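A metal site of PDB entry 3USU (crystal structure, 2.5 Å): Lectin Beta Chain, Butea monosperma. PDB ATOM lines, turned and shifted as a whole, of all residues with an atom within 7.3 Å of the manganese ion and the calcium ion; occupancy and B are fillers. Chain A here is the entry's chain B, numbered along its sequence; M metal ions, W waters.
ND1 of His 143 sits at hydrogen-bond distance from O of Asp 141. The side-chain carboxylate (OE2) of Glu 127 sits close to the side-chain hydroxyl (OG) of Ser 153 (3.1 Å). The backbone carbonyl oxygen of Gly 145 lies within hydrogen-bond range of the backbone NH of Glu 127, at 2.8 Å.
Within 4 Å of the manganese ion: Glu 127, Asp 129, Asp 138 and His 143. The nearest printed residue that does not touch the manganese ion is Ser 153 (4.1 Å).
The manganese ion is bound by NE2 of His 143 (2.1 Å), OE2 of Glu 127 (2.1 Å), OD2 of Asp 129 (2.1 Å), water W3 (2.3 Å), OD1 of Asp 138 (2.3 Å) and water W4 (2.4 Å). The manganese ion has six donor atoms within binding distance.
The calcium ion is bound by the side-chain amide nitrogen (ND2) of Asn 133 (2.2 Å), water W2 (2.2 Å), the backbone carbonyl oxygen (O) of Tyr 131 (2.2 Å), water W1 (2.3 Å), the side-chain carboxylate (OD2) of Asp 129 (2.3 Å), the side-chain carboxylate (OD1) of Asp 129 (2.4 Å) and the side-chain carboxylate (OD2) of Asp 138 (2.4 Å).
Water W3 bridges O of Ile 151 and OE1 of Glu 127.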
ATOM      1  N   ASP A  89      31.181  26.458 -28.314  1.00  0.00           N
ATOM      2  CA  ASP A  89      30.477  26.772 -27.084  1.00  0.00           C
ATOM      3  C   ASP A  89      29.938  25.482 -26.504  1.00  0.00           C
ATOM      4  O   ASP A  89      29.836  25.341 -25.283  1.00  0.00           O
ATOM      5  CB  ASP A  89      29.319  27.772 -27.354  1.00  0.00           C
ATOM      6  CG  ASP A  89      29.631  29.160 -26.878  1.00  0.00           C
ATOM      7  OD1 ASP A  89      29.764  29.334 -25.650  1.00  0.00           O
ATOM      8  OD2 ASP A  89      29.765  30.090 -27.714  1.00  0.00           O
ATOM      9  N   GLY A  90      29.563  24.570 -27.393  1.00  0.00           N
ATOM     10  CA  GLY A  90      29.339  23.182 -27.055  1.00  0.00           C
ATOM     11  C   GLY A  90      28.384  22.496 -28.013  1.00  0.00           C
ATOM     12  O   GLY A  90      28.013  23.088 -29.060  1.00  0.00           O
ATOM     13  N   ALA A 106      25.643  30.619 -29.767  1.00  0.00           N
ATOM     14  CA  ALA A 106      26.699  30.689 -28.776  1.00  0.00           C
ATOM     15  C   ALA A 106      26.425  29.785 -27.558  1.00  0.00           C
ATOM     16  O   ALA A 106      25.969  28.660 -27.739  1.00  0.00           O
ATOM     17  CB  ALA A 106      26.958  32.166 -28.406  1.00  0.00           C
ATOM     18  N   GLY A 107      26.650  30.292 -26.338  1.00  0.00           N
ATOM     19  CA  GLY A 107      26.276  29.586 -25.098  1.00  0.00           C
ATOM     20  C   GLY A 107      24.859  29.087 -24.805  1.00  0.00           C
ATOM     21  O   GLY A 107      24.690  28.277 -23.907  1.00  0.00           O
ATOM     22  N   PHE A 108      23.841  29.556 -25.522  1.00  0.00           N
ATOM     23  CA  PHE A 108      22.466  29.031 -25.413  1.00  0.00           C
ATOM     24  C   PHE A 108      22.313  27.720 -26.210  1.00  0.00           C
ATOM     25  O   PHE A 108      21.296  27.023 -26.097  1.00  0.00           O
ATOM     26  CB  PHE A 108      21.421  30.033 -25.959  1.00  0.00           C
ATOM     27  CG  PHE A 108      21.566  31.413 -25.395  1.00  0.00           C
ATOM     28  CD1 PHE A 108      20.926  31.775 -24.230  1.00  0.00           C
ATOM     29  CD2 PHE A 108      22.326  32.369 -26.061  1.00  0.00           C
ATOM     30  CE1 PHE A 108      21.070  33.028 -23.718  1.00  0.00           C
ATOM     31  CE2 PHE A 108      22.456  33.647 -25.565  1.00  0.00           C
ATOM     32  CZ  PHE A 108      21.841  33.979 -24.376  1.00  0.00           C
ATOM     33  N   LEU A 109      23.291  27.453 -27.083  1.00  0.00           N
ATOM     34  CA  LEU A 109      23.465  26.135 -27.705  1.00  0.00           C
ATOM     35  C   LEU A 109      22.398  25.767 -28.744  1.00  0.00           C
ATOM     36  O   LEU A 109      22.233  24.594 -29.078  1.00  0.00           O
ATOM     37  CB  LEU A 109      23.581  25.041 -26.645  1.00  0.00           C
ATOM     38  CG  LEU A 109      24.760  25.046 -25.684  1.00  0.00           C
ATOM     39  CD1 LEU A 109      24.654  23.822 -24.785  1.00  0.00           C
ATOM     40  CD2 LEU A 109      26.083  25.023 -26.420  1.00  0.00           C
ATOM     41  N   GLU A 127      23.950  18.266 -22.307  1.00  0.00           N
ATOM     42  CA  GLU A 127      24.873  19.204 -22.929  1.00  0.00           C
ATOM     43  C   GLU A 127      26.333  18.866 -22.597  1.00  0.00           C
ATOM     44  O   GLU A 127      26.667  18.300 -21.557  1.00  0.00           O
ATOM     45  CB  GLU A 127      24.576  20.639 -22.497  1.00  0.00           C
ATOM     46  CG  GLU A 127      24.969  20.953 -21.061  1.00  0.00           C
ATOM     47  CD  GLU A 127      24.831  22.403 -20.710  1.00  0.00           C
ATOM     48  OE1 GLU A 127      23.868  23.024 -21.231  1.00  0.00           O
ATOM     49  OE2 GLU A 127      25.639  22.918 -19.906  1.00  0.00           O
ATOM     50  N   PHE A 128      27.167  19.316 -23.531  1.00  0.00           N
ATOM     51  CA  PHE A 128      28.565  19.033 -23.570  1.00  0.00           C
ATOM     52  C   PHE A 128      29.151  20.425 -23.806  1.00  0.00           C
ATOM     53  O   PHE A 128      29.302  20.873 -24.974  1.00  0.00           O
ATOM     54  CB  PHE A 128      28.853  18.045 -24.721  1.00  0.00           C
ATOM     55  CG  PHE A 128      28.191  16.701 -24.543  1.00  0.00           C
ATOM     56  CD1 PHE A 128      28.773  15.715 -23.739  1.00  0.00           C
ATOM     57  CD2 PHE A 128      26.939  16.430 -25.147  1.00  0.00           C
ATOM     58  CE1 PHE A 128      28.139  14.497 -23.538  1.00  0.00           C
ATOM     59  CE2 PHE A 128      26.309  15.203 -24.946  1.00  0.00           C
ATOM     60  CZ  PHE A 128      26.910  14.226 -24.151  1.00  0.00           C
ATOM     61  N   ASP A 129      29.442  21.102 -22.692  1.00  0.00           N
ATOM     62  CA  ASP A 129      29.653  22.542 -22.671  1.00  0.00           C
ATOM     63  C   ASP A 129      31.115  22.913 -22.563  1.00  0.00           C
ATOM     64  O   ASP A 129      31.797  22.577 -21.585  1.00  0.00           O
ATOM     65  CB  ASP A 129      28.865  23.167 -21.487  1.00  0.00           C
ATOM     66  CG  ASP A 129      28.782  24.725 -21.569  1.00  0.00           C
ATOM     67  OD1 ASP A 129      29.416  25.362 -22.418  1.00  0.00           O
ATOM     68  OD2 ASP A 129      28.081  25.322 -20.757  1.00  0.00           O
ATOM     69  N   THR A 130      31.595  23.667 -23.536  1.00  0.00           N
ATOM     70  CA  THR A 130      33.013  23.984 -23.571  1.00  0.00           C
ATOM     71  C   THR A 130      33.393  25.401 -23.151  1.00  0.00           C
ATOM     72  O   THR A 130      34.557  25.798 -23.307  1.00  0.00           O
ATOM     73  CB  THR A 130      33.602  23.749 -24.959  1.00  0.00           C
ATOM     74  OG1 THR A 130      32.842  24.515 -25.917  1.00  0.00           O
ATOM     75  CG2 THR A 130      33.575  22.244 -25.261  1.00  0.00           C
ATOM     76  N   TYR A 131      32.422  26.167 -22.668  1.00  0.00           N
ATOM     77  CA  TYR A 131      32.707  27.564 -22.341  1.00  0.00           C
ATOM     78  C   TYR A 131      31.880  28.036 -21.183  1.00  0.00           C
ATOM     79  O   TYR A 131      30.666  27.859 -21.180  1.00  0.00           O
ATOM     80  CB  TYR A 131      32.471  28.433 -23.550  1.00  0.00           C
ATOM     81  CG  TYR A 131      32.683  29.900 -23.312  1.00  0.00           C
ATOM     82  CD1 TYR A 131      33.954  30.482 -23.484  1.00  0.00           C
ATOM     83  CD2 TYR A 131      31.600  30.726 -22.950  1.00  0.00           C
ATOM     84  CE1 TYR A 131      34.154  31.828 -23.305  1.00  0.00           C
ATOM     85  CE2 TYR A 131      31.796  32.071 -22.748  1.00  0.00           C
ATOM     86  CZ  TYR A 131      33.053  32.612 -22.931  1.00  0.00           C
ATOM     87  OH  TYR A 131      33.229  33.947 -22.734  1.00  0.00           O
ATOM     88  N   GLU A 132      32.549  28.662 -20.219  1.00  0.00           N
ATOM     89  CA  GLU A 132      31.902  29.147 -19.008  1.00  0.00           C
ATOM     90  C   GLU A 132      31.093  30.430 -19.245  1.00  0.00           C
ATOM     91  O   GLU A 132      31.607  31.567 -19.289  1.00  0.00           O
ATOM     92  CB  GLU A 132      32.929  29.365 -17.917  1.00  0.00           C
ATOM     93  CG  GLU A 132      32.350  29.283 -16.526  1.00  0.00           C
ATOM     94  CD  GLU A 132      33.325  29.754 -15.450  1.00  0.00           C
ATOM     95  OE1 GLU A 132      34.482  30.147 -15.769  1.00  0.00           O
ATOM     96  OE2 GLU A 132      32.945  29.709 -14.259  1.00  0.00           O
ATOM     97  N   ASN A 133      29.790  30.244 -19.393  1.00  0.00           N
ATOM     98  CA  ASN A 133      28.884  31.346 -19.331  1.00  0.00           C
ATOM     99  C   ASN A 133      28.639  31.555 -17.851  1.00  0.00           C
ATOM    100  O   ASN A 133      27.855  30.841 -17.221  1.00  0.00           O
ATOM    101  CB  ASN A 133      27.620  31.037 -20.088  1.00  0.00           C
ATOM    102  CG  ASN A 133      27.887  30.784 -21.550  1.00  0.00           C
ATOM    103  OD1 ASN A 133      27.925  31.727 -22.340  1.00  0.00           O
ATOM    104  ND2 ASN A 133      28.074  29.523 -21.936  1.00  0.00           N
ATOM    105  N   THR A 134      29.375  32.519 -17.293  1.00  0.00           N
ATOM    106  CA  THR A 134      29.245  32.943 -15.918  1.00  0.00           C
ATOM    107  C   THR A 134      27.794  33.298 -15.598  1.00  0.00           C
ATOM    108  O   THR A 134      27.307  33.027 -14.508  1.00  0.00           O
ATOM    109  CB  THR A 134      30.188  34.145 -15.621  1.00  0.00           C
ATOM    110  OG1 THR A 134      30.430  34.204 -14.238  1.00  0.00           O
ATOM    111  CG2 THR A 134      29.612  35.497 -16.020  1.00  0.00           C
ATOM    112  N   PHE A 136      25.144  32.055 -16.733  1.00  0.00           N
ATOM    113  CA  PHE A 136      24.314  30.864 -16.717  1.00  0.00           C
ATOM    114  C   PHE A 136      24.653  29.953 -15.544  1.00  0.00           C
ATOM    115  O   PHE A 136      24.246  28.766 -15.522  1.00  0.00           O
ATOM    116  CB  PHE A 136      24.467  30.045 -18.012  1.00  0.00           C
ATOM    117  CG  PHE A 136      24.107  30.783 -19.280  1.00  0.00           C
ATOM    118  CD1 PHE A 136      23.244  31.903 -19.257  1.00  0.00           C
ATOM    119  CD2 PHE A 136      24.602  30.369 -20.497  1.00  0.00           C
ATOM    120  CE1 PHE A 136      22.921  32.589 -20.408  1.00  0.00           C
ATOM    121  CE2 PHE A 136      24.278  31.055 -21.649  1.00  0.00           C
ATOM    122  CZ  PHE A 136      23.450  32.170 -21.613  1.00  0.00           C
ATOM    123  N   LEU A 137      25.380  30.507 -14.583  1.00  0.00           N
ATOM    124  CA  LEU A 137      25.950  29.726 -13.464  1.00  0.00           C
ATOM    125  C   LEU A 137      26.698  28.473 -13.945  1.00  0.00           C
ATOM    126  O   LEU A 137      26.556  27.420 -13.388  1.00  0.00           O
ATOM    127  CB  LEU A 137      24.893  29.413 -12.375  1.00  0.00           C
ATOM    128  CG  LEU A 137      25.374  28.944 -10.968  1.00  0.00           C
ATOM    129  CD1 LEU A 137      26.639  29.659 -10.478  1.00  0.00           C
ATOM    130  CD2 LEU A 137      24.315  28.956  -9.846  1.00  0.00           C
ATOM    131  N   ASP A 138      27.494  28.628 -15.012  1.00  0.00           N
ATOM    132  CA  ASP A 138      28.371  27.566 -15.568  1.00  0.00           C
ATOM    133  C   ASP A 138      29.551  27.212 -14.650  1.00  0.00           C
ATOM    134  O   ASP A 138      30.246  28.094 -14.188  1.00  0.00           O
ATOM    135  CB  ASP A 138      28.956  27.988 -16.927  1.00  0.00           C
ATOM    136  CG  ASP A 138      28.242  27.323 -18.134  1.00  0.00           C
ATOM    137  OD1 ASP A 138      27.449  26.315 -17.967  1.00  0.00           O
ATOM    138  OD2 ASP A 138      28.480  27.825 -19.269  1.00  0.00           O
ATOM    139  N   PRO A 139      29.821  25.923 -14.419  1.00  0.00           N
ATOM    140  CA  PRO A 139      31.005  25.610 -13.577  1.00  0.00           C
ATOM    141  C   PRO A 139      32.343  26.034 -14.229  1.00  0.00           C
ATOM    142  O   PRO A 139      32.409  26.304 -15.439  1.00  0.00           O
ATOM    143  CB  PRO A 139      30.931  24.106 -13.392  1.00  0.00           C
ATOM    144  CG  PRO A 139      30.125  23.611 -14.554  1.00  0.00           C
ATOM    145  CD  PRO A 139      29.171  24.702 -14.950  1.00  0.00           C
ATOM    146  N   ASP A 141      34.838  24.817 -15.645  1.00  0.00           N
ATOM    147  CA  ASP A 141      35.451  23.706 -16.331  1.00  0.00           C
ATOM    148  C   ASP A 141      34.502  23.325 -17.425  1.00  0.00           C
ATOM    149  O   ASP A 141      33.316  23.602 -17.340  1.00  0.00           O
ATOM    150  CB  ASP A 141      35.775  22.551 -15.362  1.00  0.00           C
ATOM    151  CG  ASP A 141      34.655  22.267 -14.380  1.00  0.00           C
ATOM    152  OD1 ASP A 141      33.900  21.284 -14.594  1.00  0.00           O
ATOM    153  OD2 ASP A 141      34.506  23.043 -13.408  1.00  0.00           O
ATOM    154  N   HIS A 143      32.141  20.819 -19.037  1.00  0.00           N
ATOM    155  CA  HIS A 143      31.269  19.965 -18.219  1.00  0.00           C
ATOM    156  C   HIS A 143      30.283  19.239 -19.043  1.00  0.00           C
ATOM    157  O   HIS A 143      30.129  19.575 -20.170  1.00  0.00           O
ATOM    158  CB  HIS A 143      30.551  20.793 -17.179  1.00  0.00           C
ATOM    159  CG  HIS A 143      29.896  22.051 -17.721  1.00  0.00           C
ATOM    160  ND1 HIS A 143      30.600  23.151 -18.021  1.00  0.00           N
ATOM    161  CD2 HIS A 143      28.559  22.368 -17.937  1.00  0.00           C
ATOM    162  CE1 HIS A 143      29.762  24.122 -18.390  1.00  0.00           C
ATOM    163  NE2 HIS A 143      28.521  23.645 -18.357  1.00  0.00           N
ATOM    164  N   ILE A 144      29.634  18.205 -18.511  1.00  0.00           N
ATOM    165  CA  ILE A 144      28.428  17.655 -19.127  1.00  0.00           C
ATOM    166  C   ILE A 144      27.316  18.125 -18.231  1.00  0.00           C
ATOM    167  O   ILE A 144      27.530  18.236 -17.037  1.00  0.00           O
ATOM    168  CB  ILE A 144      28.378  16.136 -19.163  1.00  0.00           C
ATOM    169  CG1 ILE A 144      29.519  15.583 -20.009  1.00  0.00           C
ATOM    170  CG2 ILE A 144      27.042  15.670 -19.738  1.00  0.00           C
ATOM    171  CD1 ILE A 144      29.884  14.154 -19.720  1.00  0.00           C
ATOM    172  N   GLY A 145      26.149  18.455 -18.806  1.00  0.00           N
ATOM    173  CA  GLY A 145      25.065  18.968 -17.980  1.00  0.00           C
ATOM    174  C   GLY A 145      23.715  18.418 -18.382  1.00  0.00           C
ATOM    175  O   GLY A 145      23.490  18.214 -19.574  1.00  0.00           O
ATOM    176  N   ASP A 147      19.971  19.681 -18.633  1.00  0.00           N
ATOM    177  CA  ASP A 147      19.260  20.957 -18.704  1.00  0.00           C
ATOM    178  C   ASP A 147      17.794  20.663 -18.961  1.00  0.00           C
ATOM    179  O   ASP A 147      17.438  19.945 -19.905  1.00  0.00           O
ATOM    180  CB  ASP A 147      19.698  21.830 -19.921  1.00  0.00           C
ATOM    181  CG  ASP A 147      21.191  22.138 -19.966  1.00  0.00           C
ATOM    182  OD1 ASP A 147      21.952  21.862 -19.012  1.00  0.00           O
ATOM    183  OD2 ASP A 147      21.631  22.645 -21.019  1.00  0.00           O
ATOM    184  N   ILE A 151      19.225  26.841 -19.831  1.00  0.00           N
ATOM    185  CA  ILE A 151      20.635  26.579 -20.129  1.00  0.00           C
ATOM    186  C   ILE A 151      21.432  26.468 -18.809  1.00  0.00           C
ATOM    187  O   ILE A 151      22.615  26.043 -18.759  1.00  0.00           O
ATOM    188  CB  ILE A 151      21.198  27.677 -21.061  1.00  0.00           C
ATOM    189  CG1 ILE A 151      22.663  27.389 -21.481  1.00  0.00           C
ATOM    190  CG2 ILE A 151      20.989  29.076 -20.466  1.00  0.00           C
ATOM    191  CD1 ILE A 151      22.831  26.284 -22.500  1.00  0.00           C
ATOM    192  N   LYS A 152      20.753  26.861 -17.729  1.00  0.00           N
ATOM    193  CA  LYS A 152      21.207  26.655 -16.354  1.00  0.00           C
ATOM    194  C   LYS A 152      21.032  25.163 -15.945  1.00  0.00           C
ATOM    195  O   LYS A 152      19.972  24.751 -15.451  1.00  0.00           O
ATOM    196  CB  LYS A 152      20.441  27.598 -15.408  1.00  0.00           C
ATOM    197  CG  LYS A 152      21.272  28.405 -14.406  1.00  0.00           C
ATOM    198  CD  LYS A 152      22.055  27.505 -13.457  1.00  0.00           C
ATOM    199  CE  LYS A 152      21.146  26.776 -12.485  1.00  0.00           C
ATOM    200  NZ  LYS A 152      20.713  27.680 -11.383  1.00  0.00           N
ATOM    201  N   SER A 153      22.064  24.354 -16.185  1.00  0.00           N
ATOM    202  CA  SER A 153      21.997  22.939 -15.902  1.00  0.00           C
ATOM    203  C   SER A 153      21.444  22.635 -14.521  1.00  0.00           C
ATOM    204  O   SER A 153      21.777  23.319 -13.580  1.00  0.00           O
ATOM    205  CB  SER A 153      23.352  22.293 -16.061  1.00  0.00           C
ATOM    206  OG  SER A 153      23.807  22.464 -17.389  1.00  0.00           O
ATOM    207  N   THR A 156      25.570  19.251 -13.019  1.00  0.00           N
ATOM    208  CA  THR A 156      26.690  19.006 -13.929  1.00  0.00           C
ATOM    209  C   THR A 156      27.740  18.029 -13.372  1.00  0.00           C
ATOM    210  O   THR A 156      27.765  17.747 -12.172  1.00  0.00           O
ATOM    211  CB  THR A 156      27.407  20.304 -14.341  1.00  0.00           C
ATOM    212  OG1 THR A 156      27.918  20.924 -13.176  1.00  0.00           O
ATOM    213  CG2 THR A 156      26.467  21.320 -15.115  1.00  0.00           C
HETATM  214 MN    MN M   1      26.830  24.534 -19.235  1.00  0.00          MN
HETATM  215 CA    CA M   2      28.506  27.416 -21.621  1.00  0.00          CA
HETATM  216  O   HOH W   1      28.537  27.662 -23.859  1.00  0.00           O
HETATM  217  O   HOH W   2      26.329  27.228 -21.630  1.00  0.00           O
HETATM  218  O   HOH W   3      25.097  25.777 -20.010  1.00  0.00           O
HETATM  219  O   HOH W   4      25.662  24.097 -17.239  1.00  0.00           O
